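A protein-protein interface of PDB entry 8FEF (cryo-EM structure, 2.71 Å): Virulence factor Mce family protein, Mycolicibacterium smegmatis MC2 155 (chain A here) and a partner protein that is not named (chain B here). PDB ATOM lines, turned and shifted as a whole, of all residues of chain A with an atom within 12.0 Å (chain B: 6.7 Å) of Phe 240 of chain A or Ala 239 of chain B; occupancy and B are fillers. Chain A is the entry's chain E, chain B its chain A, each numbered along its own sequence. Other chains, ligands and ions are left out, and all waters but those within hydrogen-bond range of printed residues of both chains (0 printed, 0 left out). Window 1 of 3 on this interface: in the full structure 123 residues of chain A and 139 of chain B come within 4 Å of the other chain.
Of the 22 printed residues of chain A, 7 touch a printed residue of chain B.
Along chain A the printed residues that touch a printed residue of chain B span positions 229 to 243.
Printed residues of chain B that touch a printed residue of chain A: Asp 234, Leu 236, Asp 237, Ala 239, Val 240, Ala 243, Arg 244 and Asn 247.
Among the printed residues, Asp or Glu carboxylates within 4 Å of a Lys or Arg side-chain nitrogen of the other chain: Arg 229 of chain A with Asp 234 of chain B, Arg 235 of chain A with Asp 237 of chain B and Glu 239 of chain A with Arg 244 of chain B.
The guanidinium group of Arg 229 of chain A lies within salt-bridge range of the side-chain carboxylate of Asp 234 of chain B, 2.6 Å away.
The side-chain hydroxyl of Thr 232 of chain A lies within hydrogen-bond range of the side-chain carboxylate of Asp 237 of chain B, at 2.5 Å.
The side-chain carboxylate (OD1) of Asp 237 of chain B lies within salt-bridge range of the guanidinium group (NH1) of Arg 235 of chain A (2.5 Å).
NE of Arg 244 of chain B lies within salt-bridge range of OE2 of Glu 239 of chain A (2.8 Å).
The side-chain amide nitrogen of Asn 247 of chain B sits at hydrogen-bond distance from the backbone carbonyl oxygen of Glu 239 of chain A.
OE1 of Glu 239 of chain A lies close to O of Val 240 of chain B (2.9 Å).
Among the printed residues, merely in contact across the chains: Phe 240 of chain A with Ala 239 of chain B, Leu 243 of chain A with Asn 247 of chain B, Val 236 of chain A with Val 240 of chain B, Arg 235 of chain A with Val 240 of chain B, Val 236 of chain A with Leu 236 of chain B, Leu 243 of chain A with Ala 243 of chain B, Thr 232 of chain A with Leu 236 of chain B and Phe 240 of chain A with Val 240 of chain B.
The side-chain amide nitrogen (ND2) of Asn 238 of chain B is in hydrogen-bond range of the backbone carbonyl oxygen (O) of Asp 234 of chain B (3.3 Å).
The side-chain hydroxyl (OG1) of Thr 241 of chain B lies within hydrogen-bond range of the backbone carbonyl oxygen (O) of Asp 237 of chain B (3.5 Å).
The backbone carbonyl oxygen (O) of Ala 243 of chain B is in hydrogen-bond range of the side-chain amide nitrogen (ND2) of Asn 247 of chain B.
The side-chain hydroxyl of Thr 238 of chain A sits at hydrogen-bond distance from the backbone carbonyl oxygen of Arg 235 of chain A, 2.7 Å away.
Printed residues of chain B within 4 Å of Thr 232 of chain A: Leu 236 and Asp 237.
Of the printed residues of chain B, Phe 240 of chain A touches Ala 239 (3.6 Å) and Val 240 (3.99 Å).
Of the printed residues of chain B, Leu 243 of chain A touches Ala 243 (3.8 Å) and Asn 247 (3.6 Å).
Of the printed residues of chain A, Asp 234 of chain B touches Arg 229 (2.6 Å).
No residue of chain A comes within 4 Å of Gly 235 of chain B.
Of the printed residues of chain A, Leu 236 of chain B touches Thr 232 (3.8 Å) and Val 236 (3.7 Å).
Of chain A, only Thr 232 and Arg 235 come within 4 Å of Asp 237 of chain B.
No residue of chain A comes within 4 Å of Asn 238 of chain B.
Ala 239 of chain B touches just one residue of chain A: Phe 240.
No residue of chain A comes within 4 Å of Thr 241 of chain B.
The nearest printed residue of chain B that does not touch Val 236 of chain A is Asp 237 of chain B (5.3 Å).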
ATOM      1  N   ARG A 229       9.817  33.744  20.647  1.00  0.00           N
ATOM      2  CA  ARG A 229      10.246  32.395  20.275  1.00  0.00           C
ATOM      3  C   ARG A 229       9.845  32.044  18.843  1.00  0.00           C
ATOM      4  O   ARG A 229       9.876  30.866  18.460  1.00  0.00           O
ATOM      5  CB  ARG A 229       9.694  31.358  21.253  1.00  0.00           C
ATOM      6  CG  ARG A 229      10.067  31.618  22.700  1.00  0.00           C
ATOM      7  CD  ARG A 229      11.571  31.707  22.877  1.00  0.00           C
ATOM      8  NE  ARG A 229      11.959  31.543  24.272  1.00  0.00           N
ATOM      9  CZ  ARG A 229      12.338  30.393  24.813  1.00  0.00           C
ATOM     10  NH1 ARG A 229      12.422  29.287  24.094  1.00  0.00           N
ATOM     11  NH2 ARG A 229      12.644  30.355  26.106  1.00  0.00           N
ATOM     12  N   ASN A 230       9.393  33.044  18.080  1.00  0.00           N
ATOM     13  CA  ASN A 230       9.083  32.895  16.657  1.00  0.00           C
ATOM     14  C   ASN A 230      10.153  32.134  15.879  1.00  0.00           C
ATOM     15  O   ASN A 230       9.829  31.420  14.924  1.00  0.00           O
ATOM     16  CB  ASN A 230       8.875  34.284  16.047  1.00  0.00           C
ATOM     17  CG  ASN A 230       8.542  34.237  14.572  1.00  0.00           C
ATOM     18  OD1 ASN A 230       7.944  33.279  14.088  1.00  0.00           O
ATOM     19  ND2 ASN A 230       8.927  35.280  13.849  1.00  0.00           N
ATOM     20  N   ASP A 231      11.427  32.273  16.256  1.00  0.00           N
ATOM     21  CA  ASP A 231      12.485  31.533  15.572  1.00  0.00           C
ATOM     22  C   ASP A 231      12.301  30.031  15.752  1.00  0.00           C
ATOM     23  O   ASP A 231      12.350  29.260  14.783  1.00  0.00           O
ATOM     24  CB  ASP A 231      13.854  31.975  16.090  1.00  0.00           C
ATOM     25  CG  ASP A 231      13.964  33.479  16.237  1.00  0.00           C
ATOM     26  OD1 ASP A 231      12.944  34.173  16.049  1.00  0.00           O
ATOM     27  OD2 ASP A 231      15.074  33.967  16.537  1.00  0.00           O
ATOM     28  N   THR A 232      12.081  29.602  16.997  1.00  0.00           N
ATOM     29  CA  THR A 232      11.808  28.196  17.272  1.00  0.00           C
ATOM     30  C   THR A 232      10.526  27.751  16.584  1.00  0.00           C
ATOM     31  O   THR A 232      10.429  26.616  16.104  1.00  0.00           O
ATOM     32  CB  THR A 232      11.705  27.975  18.780  1.00  0.00           C
ATOM     33  OG1 THR A 232      12.903  28.440  19.413  1.00  0.00           O
ATOM     34  CG2 THR A 232      11.500  26.502  19.100  1.00  0.00           C
ATOM     35  N   LEU A 233       9.529  28.637  16.539  1.00  0.00           N
ATOM     36  CA  LEU A 233       8.278  28.324  15.851  1.00  0.00           C
ATOM     37  C   LEU A 233       8.529  28.011  14.378  1.00  0.00           C
ATOM     38  O   LEU A 233       8.014  27.022  13.839  1.00  0.00           O
ATOM     39  CB  LEU A 233       7.304  29.494  16.002  1.00  0.00           C
ATOM     40  CG  LEU A 233       5.801  29.221  16.095  1.00  0.00           C
ATOM     41  CD1 LEU A 233       5.082  30.467  16.571  1.00  0.00           C
ATOM     42  CD2 LEU A 233       5.218  28.755  14.776  1.00  0.00           C
ATOM     43  N   ASP A 234       9.330  28.850  13.715  1.00  0.00           N
ATOM     44  CA  ASP A 234       9.667  28.630  12.311  1.00  0.00           C
ATOM     45  C   ASP A 234      10.455  27.338  12.129  1.00  0.00           C
ATOM     46  O   ASP A 234      10.203  26.576  11.185  1.00  0.00           O
ATOM     47  CB  ASP A 234      10.453  29.829  11.776  1.00  0.00           C
ATOM     48  CG  ASP A 234      10.466  29.902  10.257  1.00  0.00           C
ATOM     49  OD1 ASP A 234      10.718  28.874   9.596  1.00  0.00           O
ATOM     50  OD2 ASP A 234      10.220  31.001   9.720  1.00  0.00           O
ATOM     51  N   ARG A 235      11.411  27.069  13.026  1.00  0.00           N
ATOM     52  CA  ARG A 235      12.184  25.833  12.918  1.00  0.00           C
ATOM     53  C   ARG A 235      11.284  24.609  13.048  1.00  0.00           C
ATOM     54  O   ARG A 235      11.451  23.627  12.313  1.00  0.00           O
ATOM     55  CB  ARG A 235      13.290  25.794  13.971  1.00  0.00           C
ATOM     56  CG  ARG A 235      14.302  26.916  13.861  1.00  0.00           C
ATOM     57  CD  ARG A 235      15.247  26.903  15.045  1.00  0.00           C
ATOM     58  NE  ARG A 235      15.765  28.233  15.339  1.00  0.00           N
ATOM     59  CZ  ARG A 235      16.342  28.572  16.484  1.00  0.00           C
ATOM     60  NH1 ARG A 235      16.487  27.701  17.469  1.00  0.00           N
ATOM     61  NH2 ARG A 235      16.779  29.818  16.645  1.00  0.00           N
ATOM     62  N   VAL A 236      10.340  24.642  13.993  1.00  0.00           N
ATOM     63  CA  VAL A 236       9.403  23.533  14.144  1.00  0.00           C
ATOM     64  C   VAL A 236       8.584  23.364  12.872  1.00  0.00           C
ATOM     65  O   VAL A 236       8.512  22.271  12.300  1.00  0.00           O
ATOM     66  CB  VAL A 236       8.494  23.754  15.367  1.00  0.00           C
ATOM     67  CG1 VAL A 236       7.364  22.739  15.376  1.00  0.00           C
ATOM     68  CG2 VAL A 236       9.292  23.658  16.651  1.00  0.00           C
ATOM     69  N   LEU A 237       7.993  24.461  12.385  1.00  0.00           N
ATOM     70  CA  LEU A 237       7.142  24.388  11.204  1.00  0.00           C
ATOM     71  C   LEU A 237       7.908  24.017   9.941  1.00  0.00           C
ATOM     72  O   LEU A 237       7.279  23.673   8.937  1.00  0.00           O
ATOM     73  CB  LEU A 237       6.412  25.713  10.996  1.00  0.00           C
ATOM     74  CG  LEU A 237       5.154  25.905  11.843  1.00  0.00           C
ATOM     75  CD1 LEU A 237       4.493  27.231  11.524  1.00  0.00           C
ATOM     76  CD2 LEU A 237       4.191  24.755  11.613  1.00  0.00           C
ATOM     77  N   THR A 238       9.240  24.076   9.965  1.00  0.00           N
ATOM     78  CA  THR A 238      10.018  23.620   8.819  1.00  0.00           C
ATOM     79  C   THR A 238      10.466  22.170   8.950  1.00  0.00           C
ATOM     80  O   THR A 238      10.478  21.438   7.956  1.00  0.00           O
ATOM     81  CB  THR A 238      11.253  24.500   8.609  1.00  0.00           C
ATOM     82  OG1 THR A 238      11.989  24.601   9.834  1.00  0.00           O
ATOM     83  CG2 THR A 238      10.863  25.882   8.125  1.00  0.00           C
ATOM     84  N   GLU A 239      10.836  21.732  10.154  1.00  0.00           N
ATOM     85  CA  GLU A 239      11.484  20.434  10.299  1.00  0.00           C
ATOM     86  C   GLU A 239      10.584  19.325  10.831  1.00  0.00           C
ATOM     87  O   GLU A 239      10.899  18.150  10.614  1.00  0.00           O
ATOM     88  CB  GLU A 239      12.714  20.568  11.203  1.00  0.00           C
ATOM     89  CG  GLU A 239      13.735  21.561  10.669  1.00  0.00           C
ATOM     90  CD  GLU A 239      15.068  21.470  11.376  1.00  0.00           C
ATOM     91  OE1 GLU A 239      15.243  20.542  12.190  1.00  0.00           O
ATOM     92  OE2 GLU A 239      15.942  22.323  11.114  1.00  0.00           O
ATOM     93  N   PHE A 240       9.491  19.644  11.523  1.00  0.00           N
ATOM     94  CA  PHE A 240       8.627  18.597  12.062  1.00  0.00           C
ATOM     95  C   PHE A 240       7.633  17.989  11.067  1.00  0.00           C
ATOM     96  O   PHE A 240       7.428  16.768  11.123  1.00  0.00           O
ATOM     97  CB  PHE A 240       7.878  19.113  13.293  1.00  0.00           C
ATOM     98  CG  PHE A 240       8.508  18.703  14.588  1.00  0.00           C
ATOM     99  CD1 PHE A 240       8.347  17.415  15.067  1.00  0.00           C
ATOM    100  CD2 PHE A 240       9.268  19.597  15.321  1.00  0.00           C
ATOM    101  CE1 PHE A 240       8.927  17.027  16.255  1.00  0.00           C
ATOM    102  CE2 PHE A 240       9.850  19.215  16.511  1.00  0.00           C
ATOM    103  CZ  PHE A 240       9.679  17.927  16.977  1.00  0.00           C
ATOM    104  N   PRO A 241       6.959  18.758  10.201  1.00  0.00           N
ATOM    105  CA  PRO A 241       5.961  18.152   9.294  1.00  0.00           C
ATOM    106  C   PRO A 241       6.526  17.024   8.441  1.00  0.00           C
ATOM    107  O   PRO A 241       5.826  16.020   8.244  1.00  0.00           O
ATOM    108  CB  PRO A 241       5.496  19.338   8.436  1.00  0.00           C
ATOM    109  CG  PRO A 241       5.621  20.483   9.332  1.00  0.00           C
ATOM    110  CD  PRO A 241       6.850  20.233  10.162  1.00  0.00           C
ATOM    111  N   PRO A 242       7.756  17.127   7.891  1.00  0.00           N
ATOM    112  CA  PRO A 242       8.290  15.951   7.174  1.00  0.00           C
ATOM    113  C   PRO A 242       8.442  14.724   8.055  1.00  0.00           C
ATOM    114  O   PRO A 242       8.138  13.606   7.617  1.00  0.00           O
ATOM    115  CB  PRO A 242       9.645  16.445   6.651  1.00  0.00           C
ATOM    116  CG  PRO A 242       9.492  17.893   6.542  1.00  0.00           C
ATOM    117  CD  PRO A 242       8.657  18.285   7.711  1.00  0.00           C
ATOM    118  N   LEU A 243       8.902  14.908   9.296  1.00  0.00           N
ATOM    119  CA  LEU A 243       9.046  13.785  10.216  1.00  0.00           C
ATOM    120  C   LEU A 243       7.697  13.151  10.526  1.00  0.00           C
ATOM    121  O   LEU A 243       7.571  11.921  10.549  1.00  0.00           O
ATOM    122  CB  LEU A 243       9.725  14.253  11.502  1.00  0.00           C
ATOM    123  CG  LEU A 243       9.989  13.190  12.567  1.00  0.00           C
ATOM    124  CD1 LEU A 243      11.100  12.259  12.119  1.00  0.00           C
ATOM    125  CD2 LEU A 243      10.326  13.838  13.897  1.00  0.00           C
ATOM    126  N   ILE A 244       6.677  13.978  10.765  1.00  0.00           N
ATOM    127  CA  ILE A 244       5.352  13.457  11.084  1.00  0.00           C
ATOM    128  C   ILE A 244       4.758  12.736   9.881  1.00  0.00           C
ATOM    129  O   ILE A 244       4.128  11.680  10.024  1.00  0.00           O
ATOM    130  CB  ILE A 244       4.442  14.594  11.584  1.00  0.00           C
ATOM    131  CG1 ILE A 244       5.002  15.179  12.881  1.00  0.00           C
ATOM    132  CG2 ILE A 244       3.028  14.096  11.801  1.00  0.00           C
ATOM    133  CD1 ILE A 244       4.143  16.262  13.488  1.00  0.00           C
ATOM    134  N   GLN A 245       4.953  13.284   8.678  1.00  0.00           N
ATOM    135  CA  GLN A 245       4.480  12.616   7.472  1.00  0.00           C
ATOM    136  C   GLN A 245       5.155  11.263   7.293  1.00  0.00           C
ATOM    137  O   GLN A 245       4.490  10.268   6.976  1.00  0.00           O
ATOM    138  CB  GLN A 245       4.725  13.499   6.249  1.00  0.00           C
ATOM    139  CG  GLN A 245       4.424  12.813   4.927  1.00  0.00           C
ATOM    140  CD  GLN A 245       4.657  13.716   3.734  1.00  0.00           C
ATOM    141  OE1 GLN A 245       4.990  14.891   3.884  1.00  0.00           O
ATOM    142  NE2 GLN A 245       4.484  13.168   2.538  1.00  0.00           N
ATOM    143  N   HIS A 246       6.473  11.203   7.498  1.00  0.00           N
ATOM    144  CA  HIS A 246       7.176   9.930   7.374  1.00  0.00           C
ATOM    145  C   HIS A 246       6.687   8.926   8.408  1.00  0.00           C
ATOM    146  O   HIS A 246       6.474   7.753   8.085  1.00  0.00           O
ATOM    147  CB  HIS A 246       8.682  10.130   7.511  1.00  0.00           C
ATOM    148  CG  HIS A 246       9.456   8.849   7.481  1.00  0.00           C
ATOM    149  ND1 HIS A 246       9.429   7.990   6.403  1.00  0.00           N
ATOM    150  CD2 HIS A 246      10.267   8.275   8.400  1.00  0.00           C
ATOM    151  CE1 HIS A 246      10.196   6.945   6.657  1.00  0.00           C
ATOM    152  NE2 HIS A 246      10.717   7.094   7.862  1.00  0.00           N
ATOM    153  N   PHE A 247       6.496   9.370   9.654  1.00  0.00           N
ATOM    154  CA  PHE A 247       6.014   8.470  10.697  1.00  0.00           C
ATOM    155  C   PHE A 247       4.626   7.939  10.367  1.00  0.00           C
ATOM    156  O   PHE A 247       4.337   6.758  10.588  1.00  0.00           O
ATOM    157  CB  PHE A 247       6.011   9.181  12.050  1.00  0.00           C
ATOM    158  CG  PHE A 247       7.364   9.274  12.692  1.00  0.00           C
ATOM    159  CD1 PHE A 247       8.441   8.570  12.179  1.00  0.00           C
ATOM    160  CD2 PHE A 247       7.557  10.054  13.818  1.00  0.00           C
ATOM    161  CE1 PHE A 247       9.685   8.652  12.773  1.00  0.00           C
ATOM    162  CE2 PHE A 247       8.798  10.139  14.415  1.00  0.00           C
ATOM    163  CZ  PHE A 247       9.863   9.436  13.893  1.00  0.00           C
ATOM    164  N   ALA A 248       3.750   8.802   9.845  1.00  0.00           N
ATOM    165  CA  ALA A 248       2.435   8.349   9.409  1.00  0.00           C
ATOM    166  C   ALA A 248       2.539   7.361   8.257  1.00  0.00           C
ATOM    167  O   ALA A 248       1.709   6.453   8.141  1.00  0.00           O
ATOM    168  CB  ALA A 248       1.573   9.544   9.005  1.00  0.00           C
ATOM    169  N   GLU A 249       3.538   7.527   7.387  1.00  0.00           N
ATOM    170  CA  GLU A 249       3.718   6.586   6.285  1.00  0.00           C
ATOM    171  C   GLU A 249       4.139   5.206   6.780  1.00  0.00           C
ATOM    172  O   GLU A 249       3.733   4.189   6.204  1.00  0.00           O
ATOM    173  CB  GLU A 249       4.740   7.132   5.288  1.00  0.00           C
ATOM    174  CG  GLU A 249       4.244   8.303   4.453  1.00  0.00           C
ATOM    175  CD  GLU A 249       3.225   7.890   3.407  1.00  0.00           C
ATOM    176  OE1 GLU A 249       3.191   6.697   3.043  1.00  0.00           O
ATOM    177  OE2 GLU A 249       2.458   8.763   2.947  1.00  0.00           O
ATOM    178  N   THR A 250       4.948   5.142   7.840  1.00  0.00           N
ATOM    179  CA  THR A 250       5.514   3.879   8.306  1.00  0.00           C
ATOM    180  C   THR A 250       5.031   3.507   9.708  1.00  0.00           C
ATOM    181  O   THR A 250       5.753   2.859  10.469  1.00  0.00           O
ATOM    182  CB  THR A 250       7.043   3.926   8.252  1.00  0.00           C
ATOM    183  OG1 THR A 250       7.577   2.666   8.670  1.00  0.00           O
ATOM    184  CG2 THR A 250       7.596   5.023   9.151  1.00  0.00           C
ATOM    185  N   ASP B 234      11.793  25.667  24.555  1.00  0.00           N
ATOM    186  CA  ASP B 234      13.119  25.059  24.658  1.00  0.00           C
ATOM    187  C   ASP B 234      13.080  23.592  24.238  1.00  0.00           C
ATOM    188  O   ASP B 234      13.966  23.114  23.505  1.00  0.00           O
ATOM    189  CB  ASP B 234      13.654  25.201  26.082  1.00  0.00           C
ATOM    190  CG  ASP B 234      13.775  26.647  26.516  1.00  0.00           C
ATOM    191  OD1 ASP B 234      13.437  27.540  25.713  1.00  0.00           O
ATOM    192  OD2 ASP B 234      14.207  26.892  27.661  1.00  0.00           O
ATOM    193  N   GLY B 235      12.053  22.865  24.686  1.00  0.00           N
ATOM    194  CA  GLY B 235      11.878  21.498  24.240  1.00  0.00           C
ATOM    195  C   GLY B 235      11.664  21.401  22.745  1.00  0.00           C
ATOM    196  O   GLY B 235      12.125  20.460  22.108  1.00  0.00           O
ATOM    197  N   LEU B 236      10.970  22.382  22.163  1.00  0.00           N
ATOM    198  CA  LEU B 236      10.760  22.381  20.720  1.00  0.00           C
ATOM    199  C   LEU B 236      12.056  22.656  19.968  1.00  0.00           C
ATOM    200  O   LEU B 236      12.274  22.097  18.893  1.00  0.00           O
ATOM    201  CB  LEU B 236       9.685  23.397  20.337  1.00  0.00           C
ATOM    202  CG  LEU B 236       8.235  22.981  20.600  1.00  0.00           C
ATOM    203  CD1 LEU B 236       7.267  24.028  20.073  1.00  0.00           C
ATOM    204  CD2 LEU B 236       7.942  21.620  19.989  1.00  0.00           C
ATOM    205  N   ASP B 237      12.929  23.504  20.514  1.00  0.00           N
ATOM    206  CA  ASP B 237      14.239  23.721  19.895  1.00  0.00           C
ATOM    207  C   ASP B 237      15.058  22.435  19.877  1.00  0.00           C
ATOM    208  O   ASP B 237      15.582  22.019  18.830  1.00  0.00           O
ATOM    209  CB  ASP B 237      14.999  24.815  20.644  1.00  0.00           C
ATOM    210  CG  ASP B 237      14.801  26.182  20.035  1.00  0.00           C
ATOM    211  OD1 ASP B 237      14.839  26.291  18.793  1.00  0.00           O
ATOM    212  OD2 ASP B 237      14.608  27.151  20.798  1.00  0.00           O
ATOM    213  N   ASN B 238      15.182  21.787  21.034  1.00  0.00           N
ATOM    214  CA  ASN B 238      15.974  20.563  21.073  1.00  0.00           C
ATOM    215  C   ASN B 238      15.297  19.431  20.301  1.00  0.00           C
ATOM    216  O   ASN B 238      15.977  18.571  19.719  1.00  0.00           O
ATOM    217  CB  ASN B 238      16.246  20.178  22.521  1.00  0.00           C
ATOM    218  CG  ASN B 238      17.033  21.241  23.265  1.00  0.00           C
ATOM    219  OD1 ASN B 238      17.956  21.841  22.717  1.00  0.00           O
ATOM    220  ND2 ASN B 238      16.662  21.486  24.515  1.00  0.00           N
ATOM    221  N   ALA B 239      13.963  19.433  20.253  1.00  0.00           N
ATOM    222  CA  ALA B 239      13.237  18.472  19.438  1.00  0.00           C
ATOM    223  C   ALA B 239      13.428  18.748  17.956  1.00  0.00           C
ATOM    224  O   ALA B 239      13.413  17.814  17.156  1.00  0.00           O
ATOM    225  CB  ALA B 239      11.755  18.493  19.801  1.00  0.00           C
ATOM    226  N   VAL B 240      13.611  20.012  17.576  1.00  0.00           N
ATOM    227  CA  VAL B 240      13.972  20.344  16.202  1.00  0.00           C
ATOM    228  C   VAL B 240      15.335  19.766  15.866  1.00  0.00           C
ATOM    229  O   VAL B 240      15.541  19.211  14.780  1.00  0.00           O
ATOM    230  CB  VAL B 240      13.929  21.871  16.000  1.00  0.00           C
ATOM    231  CG1 VAL B 240      14.863  22.304  14.883  1.00  0.00           C
ATOM    232  CG2 VAL B 240      12.521  22.312  15.691  1.00  0.00           C
ATOM    233  N   THR B 241      16.286  19.881  16.796  1.00  0.00           N
ATOM    234  CA  THR B 241      17.602  19.277  16.585  1.00  0.00           C
ATOM    235  C   THR B 241      17.498  17.765  16.364  1.00  0.00           C
ATOM    236  O   THR B 241      18.000  17.228  15.365  1.00  0.00           O
ATOM    237  CB  THR B 241      18.517  19.584  17.770  1.00  0.00           C
ATOM    238  OG1 THR B 241      18.771  20.992  17.830  1.00  0.00           O
ATOM    239  CG2 THR B 241      19.834  18.842  17.631  1.00  0.00           C
ATOM    240  N   THR B 242      16.821  17.063  17.278  1.00  0.00           N
ATOM    241  CA  THR B 242      16.735  15.609  17.137  1.00  0.00           C
ATOM    242  C   THR B 242      15.844  15.195  15.965  1.00  0.00           C
ATOM    243  O   THR B 242      16.045  14.121  15.391  1.00  0.00           O
ATOM    244  CB  THR B 242      16.257  14.953  18.435  1.00  0.00           C
ATOM    245  OG1 THR B 242      16.266  13.529  18.276  1.00  0.00           O
ATOM    246  CG2 THR B 242      14.860  15.386  18.785  1.00  0.00           C
ATOM    247  N   ALA B 243      14.882  16.033  15.573  1.00  0.00           N
ATOM    248  CA  ALA B 243      14.054  15.723  14.414  1.00  0.00           C
ATOM    249  C   ALA B 243      14.837  15.895  13.123  1.00  0.00           C
ATOM    250  O   ALA B 243      14.644  15.135  12.170  1.00  0.00           O
ATOM    251  CB  ALA B 243      12.807  16.606  14.409  1.00  0.00           C
ATOM    252  N   ARG B 244      15.722  16.892  13.074  1.00  0.00           N
ATOM    253  CA  ARG B 244      16.649  17.004  11.956  1.00  0.00           C
ATOM    254  C   ARG B 244      17.538  15.772  11.876  1.00  0.00           C
ATOM    255  O   ARG B 244      17.774  15.232  10.787  1.00  0.00           O
ATOM    256  CB  ARG B 244      17.492  18.268  12.105  1.00  0.00           C
ATOM    257  CG  ARG B 244      18.174  18.728  10.834  1.00  0.00           C
ATOM    258  CD  ARG B 244      19.015  19.961  11.101  1.00  0.00           C
ATOM    259  NE  ARG B 244      18.265  20.979  11.826  1.00  0.00           N
ATOM    260  CZ  ARG B 244      18.807  22.042  12.402  1.00  0.00           C
ATOM    261  NH1 ARG B 244      20.112  22.260  12.362  1.00  0.00           N
ATOM    262  NH2 ARG B 244      18.022  22.908  13.036  1.00  0.00           N
ATOM    263  N   THR B 245      18.025  15.306  13.031  1.00  0.00           N
ATOM    264  CA  THR B 245      18.824  14.083  13.055  1.00  0.00           C
ATOM    265  C   THR B 245      18.033  12.888  12.529  1.00  0.00           C
ATOM    266  O   THR B 245      18.546  12.098  11.727  1.00  0.00           O
ATOM    267  CB  THR B 245      19.321  13.814  14.475  1.00  0.00           C
ATOM    268  OG1 THR B 245      20.347  14.756  14.801  1.00  0.00           O
ATOM    269  CG2 THR B 245      19.873  12.403  14.601  1.00  0.00           C
ATOM    270  N   ASN B 247      15.423  12.929  10.507  1.00  0.00           N
ATOM    271  CA  ASN B 247      15.162  13.105   9.081  1.00  0.00           C
ATOM    272  C   ASN B 247      16.388  12.768   8.244  1.00  0.00           C
ATOM    273  O   ASN B 247      16.263  12.191   7.159  1.00  0.00           O
ATOM    274  CB  ASN B 247      14.705  14.536   8.802  1.00  0.00           C
ATOM    275  CG  ASN B 247      13.268  14.776   9.203  1.00  0.00           C
ATOM    276  OD1 ASN B 247      12.443  13.865   9.170  1.00  0.00           O
ATOM    277  ND2 ASN B 247      12.957  16.010   9.582  1.00  0.00           N
